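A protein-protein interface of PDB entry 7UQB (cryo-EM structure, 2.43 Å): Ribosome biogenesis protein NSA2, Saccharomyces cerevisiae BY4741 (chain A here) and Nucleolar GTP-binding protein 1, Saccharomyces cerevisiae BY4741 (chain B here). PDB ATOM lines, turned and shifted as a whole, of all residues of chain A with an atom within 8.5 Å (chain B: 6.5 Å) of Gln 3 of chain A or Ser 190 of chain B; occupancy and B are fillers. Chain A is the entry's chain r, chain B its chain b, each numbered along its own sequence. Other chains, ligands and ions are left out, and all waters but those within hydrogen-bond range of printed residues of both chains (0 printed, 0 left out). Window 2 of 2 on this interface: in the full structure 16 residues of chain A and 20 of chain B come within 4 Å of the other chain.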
ATOM      1  N   PRO A   2     -32.413 -19.488 -31.556  1.00  0.00           N
ATOM      2  CA  PRO A   2     -31.070 -19.293 -31.014  1.00  0.00           C
ATOM      3  C   PRO A   2     -31.107 -19.296 -29.486  1.00  0.00           C
ATOM      4  O   PRO A   2     -32.152 -19.027 -28.900  1.00  0.00           O
ATOM      5  CB  PRO A   2     -30.675 -17.940 -31.579  1.00  0.00           C
ATOM      6  CG  PRO A   2     -31.944 -17.204 -31.619  1.00  0.00           C
ATOM      7  CD  PRO A   2     -33.030 -18.207 -31.923  1.00  0.00           C
ATOM      8  N   GLN A   3     -29.991 -19.634 -28.849  1.00  0.00           N
ATOM      9  CA  GLN A   3     -29.962 -19.812 -27.407  1.00  0.00           C
ATOM     10  C   GLN A   3     -28.663 -19.259 -26.841  1.00  0.00           C
ATOM     11  O   GLN A   3     -27.626 -19.263 -27.510  1.00  0.00           O
ATOM     12  CB  GLN A   3     -30.124 -21.292 -27.032  1.00  0.00           C
ATOM     13  CG  GLN A   3     -29.175 -22.219 -27.777  1.00  0.00           C
ATOM     14  CD  GLN A   3     -29.572 -23.677 -27.678  1.00  0.00           C
ATOM     15  OE1 GLN A   3     -30.003 -24.146 -26.628  1.00  0.00           O
ATOM     16  NE2 GLN A   3     -29.436 -24.400 -28.780  1.00  0.00           N
ATOM     17  N   ASN A   4     -28.747 -18.765 -25.606  1.00  0.00           N
ATOM     18  CA  ASN A   4     -27.609 -18.256 -24.822  1.00  0.00           C
ATOM     19  C   ASN A   4     -27.067 -17.009 -25.519  1.00  0.00           C
ATOM     20  O   ASN A   4     -27.863 -16.136 -25.900  1.00  0.00           O
ATOM     21  CB  ASN A   4     -26.611 -19.386 -24.597  1.00  0.00           C
ATOM     22  CG  ASN A   4     -27.248 -20.599 -23.944  1.00  0.00           C
ATOM     23  OD1 ASN A   4     -27.981 -20.473 -22.966  1.00  0.00           O
ATOM     24  ND2 ASN A   4     -26.992 -21.773 -24.499  1.00  0.00           N
ATOM     25  N   ASP A   5     -25.754 -16.868 -25.697  1.00  0.00           N
ATOM     26  CA  ASP A   5     -25.168 -15.651 -26.263  1.00  0.00           C
ATOM     27  C   ASP A   5     -24.932 -15.834 -27.764  1.00  0.00           C
ATOM     28  O   ASP A   5     -23.803 -15.846 -28.263  1.00  0.00           O
ATOM     29  CB  ASP A   5     -23.882 -15.296 -25.530  1.00  0.00           C
ATOM     30  CG  ASP A   5     -22.962 -16.487 -25.357  1.00  0.00           C
ATOM     31  OD1 ASP A   5     -23.473 -17.614 -25.196  1.00  0.00           O
ATOM     32  OD2 ASP A   5     -21.727 -16.299 -25.389  1.00  0.00           O
ATOM     33  N   TYR A   6     -26.044 -15.958 -28.493  1.00  0.00           N
ATOM     34  CA  TYR A   6     -25.958 -16.320 -29.903  1.00  0.00           C
ATOM     35  C   TYR A   6     -25.397 -15.192 -30.762  1.00  0.00           C
ATOM     36  O   TYR A   6     -24.704 -15.467 -31.742  1.00  0.00           O
ATOM     37  CB  TYR A   6     -27.320 -16.779 -30.428  1.00  0.00           C
ATOM     38  CG  TYR A   6     -28.509 -15.922 -30.053  1.00  0.00           C
ATOM     39  CD1 TYR A   6     -29.238 -16.182 -28.900  1.00  0.00           C
ATOM     40  CD2 TYR A   6     -28.939 -14.890 -30.881  1.00  0.00           C
ATOM     41  CE1 TYR A   6     -30.334 -15.419 -28.562  1.00  0.00           C
ATOM     42  CE2 TYR A   6     -30.038 -14.117 -30.547  1.00  0.00           C
ATOM     43  CZ  TYR A   6     -30.730 -14.388 -29.385  1.00  0.00           C
ATOM     44  OH  TYR A   6     -31.825 -13.633 -29.044  1.00  0.00           O
ATOM     45  N   ILE A   7     -25.662 -13.932 -30.413  1.00  0.00           N
ATOM     46  CA  ILE A   7     -25.094 -12.818 -31.169  1.00  0.00           C
ATOM     47  C   ILE A   7     -23.585 -12.739 -30.960  1.00  0.00           C
ATOM     48  O   ILE A   7     -22.825 -12.518 -31.910  1.00  0.00           O
ATOM     49  CB  ILE A   7     -25.799 -11.501 -30.795  1.00  0.00           C
ATOM     50  CG1 ILE A   7     -27.167 -11.415 -31.475  1.00  0.00           C
ATOM     51  CG2 ILE A   7     -24.952 -10.292 -31.168  1.00  0.00           C
ATOM     52  CD1 ILE A   7     -27.095 -11.318 -32.985  1.00  0.00           C
ATOM     53  N   GLU A   8     -23.125 -12.932 -29.720  1.00  0.00           N
ATOM     54  CA  GLU A   8     -21.688 -12.955 -29.464  1.00  0.00           C
ATOM     55  C   GLU A   8     -21.016 -14.113 -30.192  1.00  0.00           C
ATOM     56  O   GLU A   8     -19.941 -13.943 -30.778  1.00  0.00           O
ATOM     57  CB  GLU A   8     -21.416 -13.038 -27.963  1.00  0.00           C
ATOM     58  CG  GLU A   8     -21.326 -11.689 -27.279  1.00  0.00           C
ATOM     59  CD  GLU A   8     -21.192 -11.808 -25.772  1.00  0.00           C
ATOM     60  OE1 GLU A   8     -21.070 -12.946 -25.273  1.00  0.00           O
ATOM     61  OE2 GLU A   8     -21.217 -10.763 -25.087  1.00  0.00           O
ATOM     62  N   ARG A   9     -21.643 -15.293 -30.178  1.00  0.00           N
ATOM     63  CA  ARG A   9     -21.080 -16.425 -30.907  1.00  0.00           C
ATOM     64  C   ARG A   9     -21.088 -16.182 -32.413  1.00  0.00           C
ATOM     65  O   ARG A   9     -20.159 -16.592 -33.115  1.00  0.00           O
ATOM     66  CB  ARG A   9     -21.834 -17.711 -30.562  1.00  0.00           C
ATOM     67  CG  ARG A   9     -21.647 -18.164 -29.125  1.00  0.00           C
ATOM     68  CD  ARG A   9     -22.025 -19.626 -28.937  1.00  0.00           C
ATOM     69  NE  ARG A   9     -23.310 -19.953 -29.542  1.00  0.00           N
ATOM     70  CZ  ARG A   9     -24.487 -19.742 -28.969  1.00  0.00           C
ATOM     71  NH1 ARG A   9     -24.583 -19.178 -27.778  1.00  0.00           N
ATOM     72  NH2 ARG A   9     -25.593 -20.109 -29.607  1.00  0.00           N
ATOM     73  N   ARG B 159     -33.175 -15.315 -23.649  1.00  0.00           N
ATOM     74  CA  ARG B 159     -32.334 -16.141 -24.506  1.00  0.00           C
ATOM     75  C   ARG B 159     -32.144 -17.560 -23.984  1.00  0.00           C
ATOM     76  O   ARG B 159     -31.384 -18.327 -24.582  1.00  0.00           O
ATOM     77  CB  ARG B 159     -30.973 -15.474 -24.698  1.00  0.00           C
ATOM     78  CG  ARG B 159     -31.065 -14.017 -25.088  1.00  0.00           C
ATOM     79  CD  ARG B 159     -29.749 -13.506 -25.620  1.00  0.00           C
ATOM     80  NE  ARG B 159     -28.668 -13.615 -24.649  1.00  0.00           N
ATOM     81  CZ  ARG B 159     -28.301 -12.643 -23.827  1.00  0.00           C
ATOM     82  NH1 ARG B 159     -28.919 -11.475 -23.821  1.00  0.00           N
ATOM     83  NH2 ARG B 159     -27.288 -12.849 -22.992  1.00  0.00           N
ATOM     84  N   LEU B 160     -32.809 -17.928 -22.895  1.00  0.00           N
ATOM     85  CA  LEU B 160     -32.688 -19.284 -22.381  1.00  0.00           C
ATOM     86  C   LEU B 160     -33.346 -20.272 -23.341  1.00  0.00           C
ATOM     87  O   LEU B 160     -34.353 -19.946 -23.974  1.00  0.00           O
ATOM     88  CB  LEU B 160     -33.332 -19.401 -21.001  1.00  0.00           C
ATOM     89  CG  LEU B 160     -32.565 -18.853 -19.798  1.00  0.00           C
ATOM     90  CD1 LEU B 160     -33.314 -19.179 -18.519  1.00  0.00           C
ATOM     91  CD2 LEU B 160     -31.154 -19.411 -19.760  1.00  0.00           C
ATOM     92  N   PRO B 161     -32.793 -21.473 -23.485  1.00  0.00           N
ATOM     93  CA  PRO B 161     -33.451 -22.487 -24.311  1.00  0.00           C
ATOM     94  C   PRO B 161     -34.749 -22.959 -23.680  1.00  0.00           C
ATOM     95  O   PRO B 161     -34.906 -22.974 -22.458  1.00  0.00           O
ATOM     96  CB  PRO B 161     -32.420 -23.617 -24.369  1.00  0.00           C
ATOM     97  CG  PRO B 161     -31.645 -23.466 -23.108  1.00  0.00           C
ATOM     98  CD  PRO B 161     -31.554 -21.984 -22.874  1.00  0.00           C
ATOM     99  N   SER B 162     -35.691 -23.345 -24.535  1.00  0.00           N
ATOM    100  CA  SER B 162     -36.967 -23.884 -24.081  1.00  0.00           C
ATOM    101  C   SER B 162     -36.794 -25.379 -23.841  1.00  0.00           C
ATOM    102  O   SER B 162     -36.678 -26.159 -24.792  1.00  0.00           O
ATOM    103  CB  SER B 162     -38.072 -23.615 -25.097  1.00  0.00           C
ATOM    104  OG  SER B 162     -38.041 -24.567 -26.144  1.00  0.00           O
ATOM    105  N   SER B 181     -20.291 -31.845 -26.446  1.00  0.00           N
ATOM    106  CA  SER B 181     -20.739 -30.942 -27.497  1.00  0.00           C
ATOM    107  C   SER B 181     -20.543 -31.554 -28.875  1.00  0.00           C
ATOM    108  O   SER B 181     -21.347 -31.307 -29.780  1.00  0.00           O
ATOM    109  CB  SER B 181     -20.003 -29.607 -27.396  1.00  0.00           C
ATOM    110  OG  SER B 181     -20.206 -29.010 -26.129  1.00  0.00           O
ATOM    111  N   LEU B 184     -23.525 -33.803 -29.345  1.00  0.00           N
ATOM    112  CA  LEU B 184     -24.723 -33.017 -29.631  1.00  0.00           C
ATOM    113  C   LEU B 184     -24.699 -32.473 -31.055  1.00  0.00           C
ATOM    114  O   LEU B 184     -25.731 -32.454 -31.736  1.00  0.00           O
ATOM    115  CB  LEU B 184     -24.879 -31.877 -28.625  1.00  0.00           C
ATOM    116  CG  LEU B 184     -26.254 -31.202 -28.703  1.00  0.00           C
ATOM    117  CD1 LEU B 184     -27.326 -32.100 -28.105  1.00  0.00           C
ATOM    118  CD2 LEU B 184     -26.268 -29.829 -28.047  1.00  0.00           C
ATOM    119  N   ARG B 185     -23.526 -32.035 -31.524  1.00  0.00           N
ATOM    120  CA  ARG B 185     -23.380 -31.607 -32.912  1.00  0.00           C
ATOM    121  C   ARG B 185     -23.653 -32.754 -33.876  1.00  0.00           C
ATOM    122  O   ARG B 185     -24.250 -32.551 -34.939  1.00  0.00           O
ATOM    123  CB  ARG B 185     -21.975 -31.056 -33.152  1.00  0.00           C
ATOM    124  CG  ARG B 185     -21.811 -29.556 -32.974  1.00  0.00           C
ATOM    125  CD  ARG B 185     -20.469 -29.123 -33.545  1.00  0.00           C
ATOM    126  NE  ARG B 185     -20.171 -27.716 -33.307  1.00  0.00           N
ATOM    127  CZ  ARG B 185     -19.022 -27.135 -33.622  1.00  0.00           C
ATOM    128  NH1 ARG B 185     -18.041 -27.810 -34.198  1.00  0.00           N
ATOM    129  NH2 ARG B 185     -18.852 -25.844 -33.350  1.00  0.00           N
ATOM    130  N   THR B 188     -27.750 -33.623 -33.470  1.00  0.00           N
ATOM    131  CA  THR B 188     -28.714 -32.549 -33.675  1.00  0.00           C
ATOM    132  C   THR B 188     -28.080 -31.471 -34.548  1.00  0.00           C
ATOM    133  O   THR B 188     -26.920 -31.573 -34.951  1.00  0.00           O
ATOM    134  CB  THR B 188     -29.182 -31.953 -32.338  1.00  0.00           C
ATOM    135  OG1 THR B 188     -28.061 -31.398 -31.642  1.00  0.00           O
ATOM    136  CG2 THR B 188     -29.834 -33.017 -31.467  1.00  0.00           C
ATOM    137  N   LYS B 189     -28.851 -30.425 -34.844  1.00  0.00           N
ATOM    138  CA  LYS B 189     -28.331 -29.273 -35.569  1.00  0.00           C
ATOM    139  C   LYS B 189     -28.135 -28.063 -34.660  1.00  0.00           C
ATOM    140  O   LYS B 189     -28.135 -26.924 -35.136  1.00  0.00           O
ATOM    141  CB  LYS B 189     -29.233 -28.924 -36.756  1.00  0.00           C
ATOM    142  CG  LYS B 189     -30.634 -28.479 -36.400  1.00  0.00           C
ATOM    143  CD  LYS B 189     -31.428 -28.174 -37.657  1.00  0.00           C
ATOM    144  CE  LYS B 189     -31.597 -29.413 -38.519  1.00  0.00           C
ATOM    145  NZ  LYS B 189     -32.435 -29.136 -39.716  1.00  0.00           N
ATOM    146  N   SER B 190     -27.968 -28.293 -33.361  1.00  0.00           N
ATOM    147  CA  SER B 190     -27.532 -27.244 -32.456  1.00  0.00           C
ATOM    148  C   SER B 190     -26.115 -26.806 -32.810  1.00  0.00           C
ATOM    149  O   SER B 190     -25.294 -27.600 -33.275  1.00  0.00           O
ATOM    150  CB  SER B 190     -27.588 -27.735 -31.008  1.00  0.00           C
ATOM    151  OG  SER B 190     -26.954 -26.825 -30.129  1.00  0.00           O
ATOM    152  N   ASP B 191     -25.834 -25.523 -32.593  1.00  0.00           N
ATOM    153  CA  ASP B 191     -24.551 -24.928 -32.961  1.00  0.00           C
ATOM    154  C   ASP B 191     -23.636 -24.751 -31.756  1.00  0.00           C
ATOM    155  O   ASP B 191     -22.921 -23.750 -31.651  1.00  0.00           O
ATOM    156  CB  ASP B 191     -24.769 -23.595 -33.670  1.00  0.00           C
ATOM    157  CG  ASP B 191     -25.509 -22.591 -32.810  1.00  0.00           C
ATOM    158  OD1 ASP B 191     -26.324 -23.016 -31.967  1.00  0.00           O
ATOM    159  OD2 ASP B 191     -25.272 -21.377 -32.975  1.00  0.00           O
ATOM    160  N   VAL B 192     -23.644 -25.712 -30.829  1.00  0.00           N
ATOM    161  CA  VAL B 192     -22.810 -25.616 -29.638  1.00  0.00           C
ATOM    162  C   VAL B 192     -21.341 -25.720 -30.029  1.00  0.00           C
ATOM    163  O   VAL B 192     -20.955 -26.535 -30.879  1.00  0.00           O
ATOM    164  CB  VAL B 192     -23.219 -26.690 -28.611  1.00  0.00           C
ATOM    165  CG1 VAL B 192     -23.088 -28.098 -29.188  1.00  0.00           C
ATOM    166  CG2 VAL B 192     -22.422 -26.542 -27.320  1.00  0.00           C
ATOM    167  N   LEU B 204     -26.684 -24.783 -20.426  1.00  0.00           N
ATOM    168  CA  LEU B 204     -27.392 -25.872 -21.084  1.00  0.00           C
ATOM    169  C   LEU B 204     -27.657 -25.533 -22.546  1.00  0.00           C
ATOM    170  O   LEU B 204     -28.052 -24.412 -22.878  1.00  0.00           O
ATOM    171  CB  LEU B 204     -28.709 -26.151 -20.364  1.00  0.00           C
ATOM    172  CG  LEU B 204     -28.640 -26.299 -18.843  1.00  0.00           C
ATOM    173  CD1 LEU B 204     -30.031 -26.259 -18.243  1.00  0.00           C
ATOM    174  CD2 LEU B 204     -27.931 -27.583 -18.462  1.00  0.00           C
ATOM    175  N   TYR B 205     -27.436 -26.509 -23.422  1.00  0.00           N
ATOM    176  CA  TYR B 205     -27.735 -26.382 -24.841  1.00  0.00           C
ATOM    177  C   TYR B 205     -28.690 -27.489 -25.253  1.00  0.00           C
ATOM    178  O   TYR B 205     -28.548 -28.635 -24.822  1.00  0.00           O
ATOM    179  CB  TYR B 205     -26.466 -26.444 -25.693  1.00  0.00           C
ATOM    180  CG  TYR B 205     -25.701 -25.144 -25.741  1.00  0.00           C
ATOM    181  CD1 TYR B 205     -24.895 -24.756 -24.683  1.00  0.00           C
ATOM    182  CD2 TYR B 205     -25.783 -24.305 -26.844  1.00  0.00           C
ATOM    183  CE1 TYR B 205     -24.191 -23.569 -24.719  1.00  0.00           C
ATOM    184  CE2 TYR B 205     -25.085 -23.117 -26.889  1.00  0.00           C
ATOM    185  CZ  TYR B 205     -24.289 -22.754 -25.822  1.00  0.00           C
ATOM    186  OH  TYR B 205     -23.589 -21.571 -25.854  1.00  0.00           O
ATOM    187  N   VAL B 206     -29.663 -27.150 -26.088  1.00  0.00           N
ATOM    188  CA  VAL B 206     -30.722 -28.071 -26.475  1.00  0.00           C
ATOM    189  C   VAL B 206     -30.616 -28.338 -27.967  1.00  0.00           C
ATOM    190  O   VAL B 206     -30.400 -27.413 -28.756  1.00  0.00           O
ATOM    191  CB  VAL B 206     -32.114 -27.518 -26.117  1.00  0.00           C
ATOM    192  CG1 VAL B 206     -33.200 -28.525 -26.467  1.00  0.00           C
ATOM    193  CG2 VAL B 206     -32.165 -27.180 -24.652  1.00  0.00           C
ATOM    194  N   GLY B 207     -30.723 -29.614 -28.342  1.00  0.00           N
ATOM    195  CA  GLY B 207     -30.951 -29.992 -29.716  1.00  0.00           C
ATOM    196  C   GLY B 207     -32.176 -30.884 -29.805  1.00  0.00           C
ATOM    197  O   GLY B 207     -32.714 -31.330 -28.794  1.00  0.00           O
ATOM    198  N   HIS B 208     -32.610 -31.138 -31.035  1.00  0.00           N
ATOM    199  CA  HIS B 208     -33.782 -31.967 -31.262  1.00  0.00           C
ATOM    200  C   HIS B 208     -33.504 -32.949 -32.387  1.00  0.00           C
ATOM    201  O   HIS B 208     -32.648 -32.712 -33.242  1.00  0.00           O
ATOM    202  CB  HIS B 208     -35.016 -31.123 -31.603  1.00  0.00           C
ATOM    203  CG  HIS B 208     -35.466 -30.236 -30.488  1.00  0.00           C
ATOM    204  ND1 HIS B 208     -36.375 -30.640 -29.536  1.00  0.00           N
ATOM    205  CD2 HIS B 208     -35.130 -28.965 -30.169  1.00  0.00           C
ATOM    206  CE1 HIS B 208     -36.581 -29.656 -28.680  1.00  0.00           C
ATOM    207  NE2 HIS B 208     -35.837 -28.627 -29.043  1.00  0.00           N
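O of Arg 159 of chain B lies within hydrogen-bond range of N of Asn 4 of chain A.
The guanidinium group (NH2) of Arg 9 of chain A is in salt-bridge range of the side-chain carboxylate (OD2) of Asp 191 of chain B (3.6 Å).
ND2 of Asn 4 of chain A sits at hydrogen-bond distance from O of Leu 204 of chain B, 3.3 Å away.
The guanidinium group (NH1) of Arg 9 of chain A is in hydrogen-bond range of the side-chain hydroxyl (OH) of Tyr 205 of chain B (3.2 Å).
The backbone NH (N) of Val 206 of chain B sits at hydrogen-bond distance from the side-chain amide oxygen (OE1) of Gln 3 of chain A.
The backbone carbonyl oxygen (O) of Gln 3 of chain A is in hydrogen-bond range of the guanidinium group (NH2) of Arg 9 of chain A (3.0 Å).
OD1 of Asp 5 of chain A is in salt-bridge range of NH1 of Arg 9 of chain A (3.2 Å).
Among the printed residues, pairs that only touch across the chains: Gln 3 of chain A with Arg 159 of chain B, Gln 3 of chain A with Pro 161 of chain B, Gln 3 of chain A with Ser 190 of chain B, Gln 3 of chain A with Tyr 205 of chain B, Asn 4 of chain A with Pro 161 of chain B, Asn 4 of chain A with Tyr 205 of chain B and Tyr 6 of chain A with Arg 159 of chain B.
Gln 3 of chain A touches five residues of chain B.
Ser 190 of chain B touches just one residue of chain A: Gln 3.
Printed residues of chain A within 4 Å of Pro 161 of chain B: Gln 3 (3.4 Å) and Asn 4 (3.9 Å).
Of the printed residues of chain B, Arg 9 of chain A touches Asp 191 (3.6 Å) and Tyr 205 (3.2 Å).
Printed residues of chain A within 4 Å of Leu 204 of chain B: Asn 4.
Printed residues of chain B within 4 Å of Asn 4 of chain A: Arg 159, Pro 161, Leu 204 and Tyr 205.
The nearest residue of chain A that does not touch Ser 190 of chain B is Arg 9 of chain A (6.9 Å).
Hydrophobic or aromatic side chains of chain A that line the printed part of chain B: Tyr 6.
Along chain A the printed residues that touch a printed residue of chain B span positions 3 to 9.
Of the 17 printed residues of chain B, 7 touch a printed residue of chain A.
Printed residues of chain B that touch a printed residue of chain A: Arg 159, Pro 161, Ser 190, Asp 191, Leu 204, Tyr 205 and Val 206.
Among the printed residues, Asp or Glu carboxylates within 4 Å of a Lys or Arg side-chain nitrogen of the other chain: Arg 9 of chain A with Asp 191 of chain B (3.6 Å).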
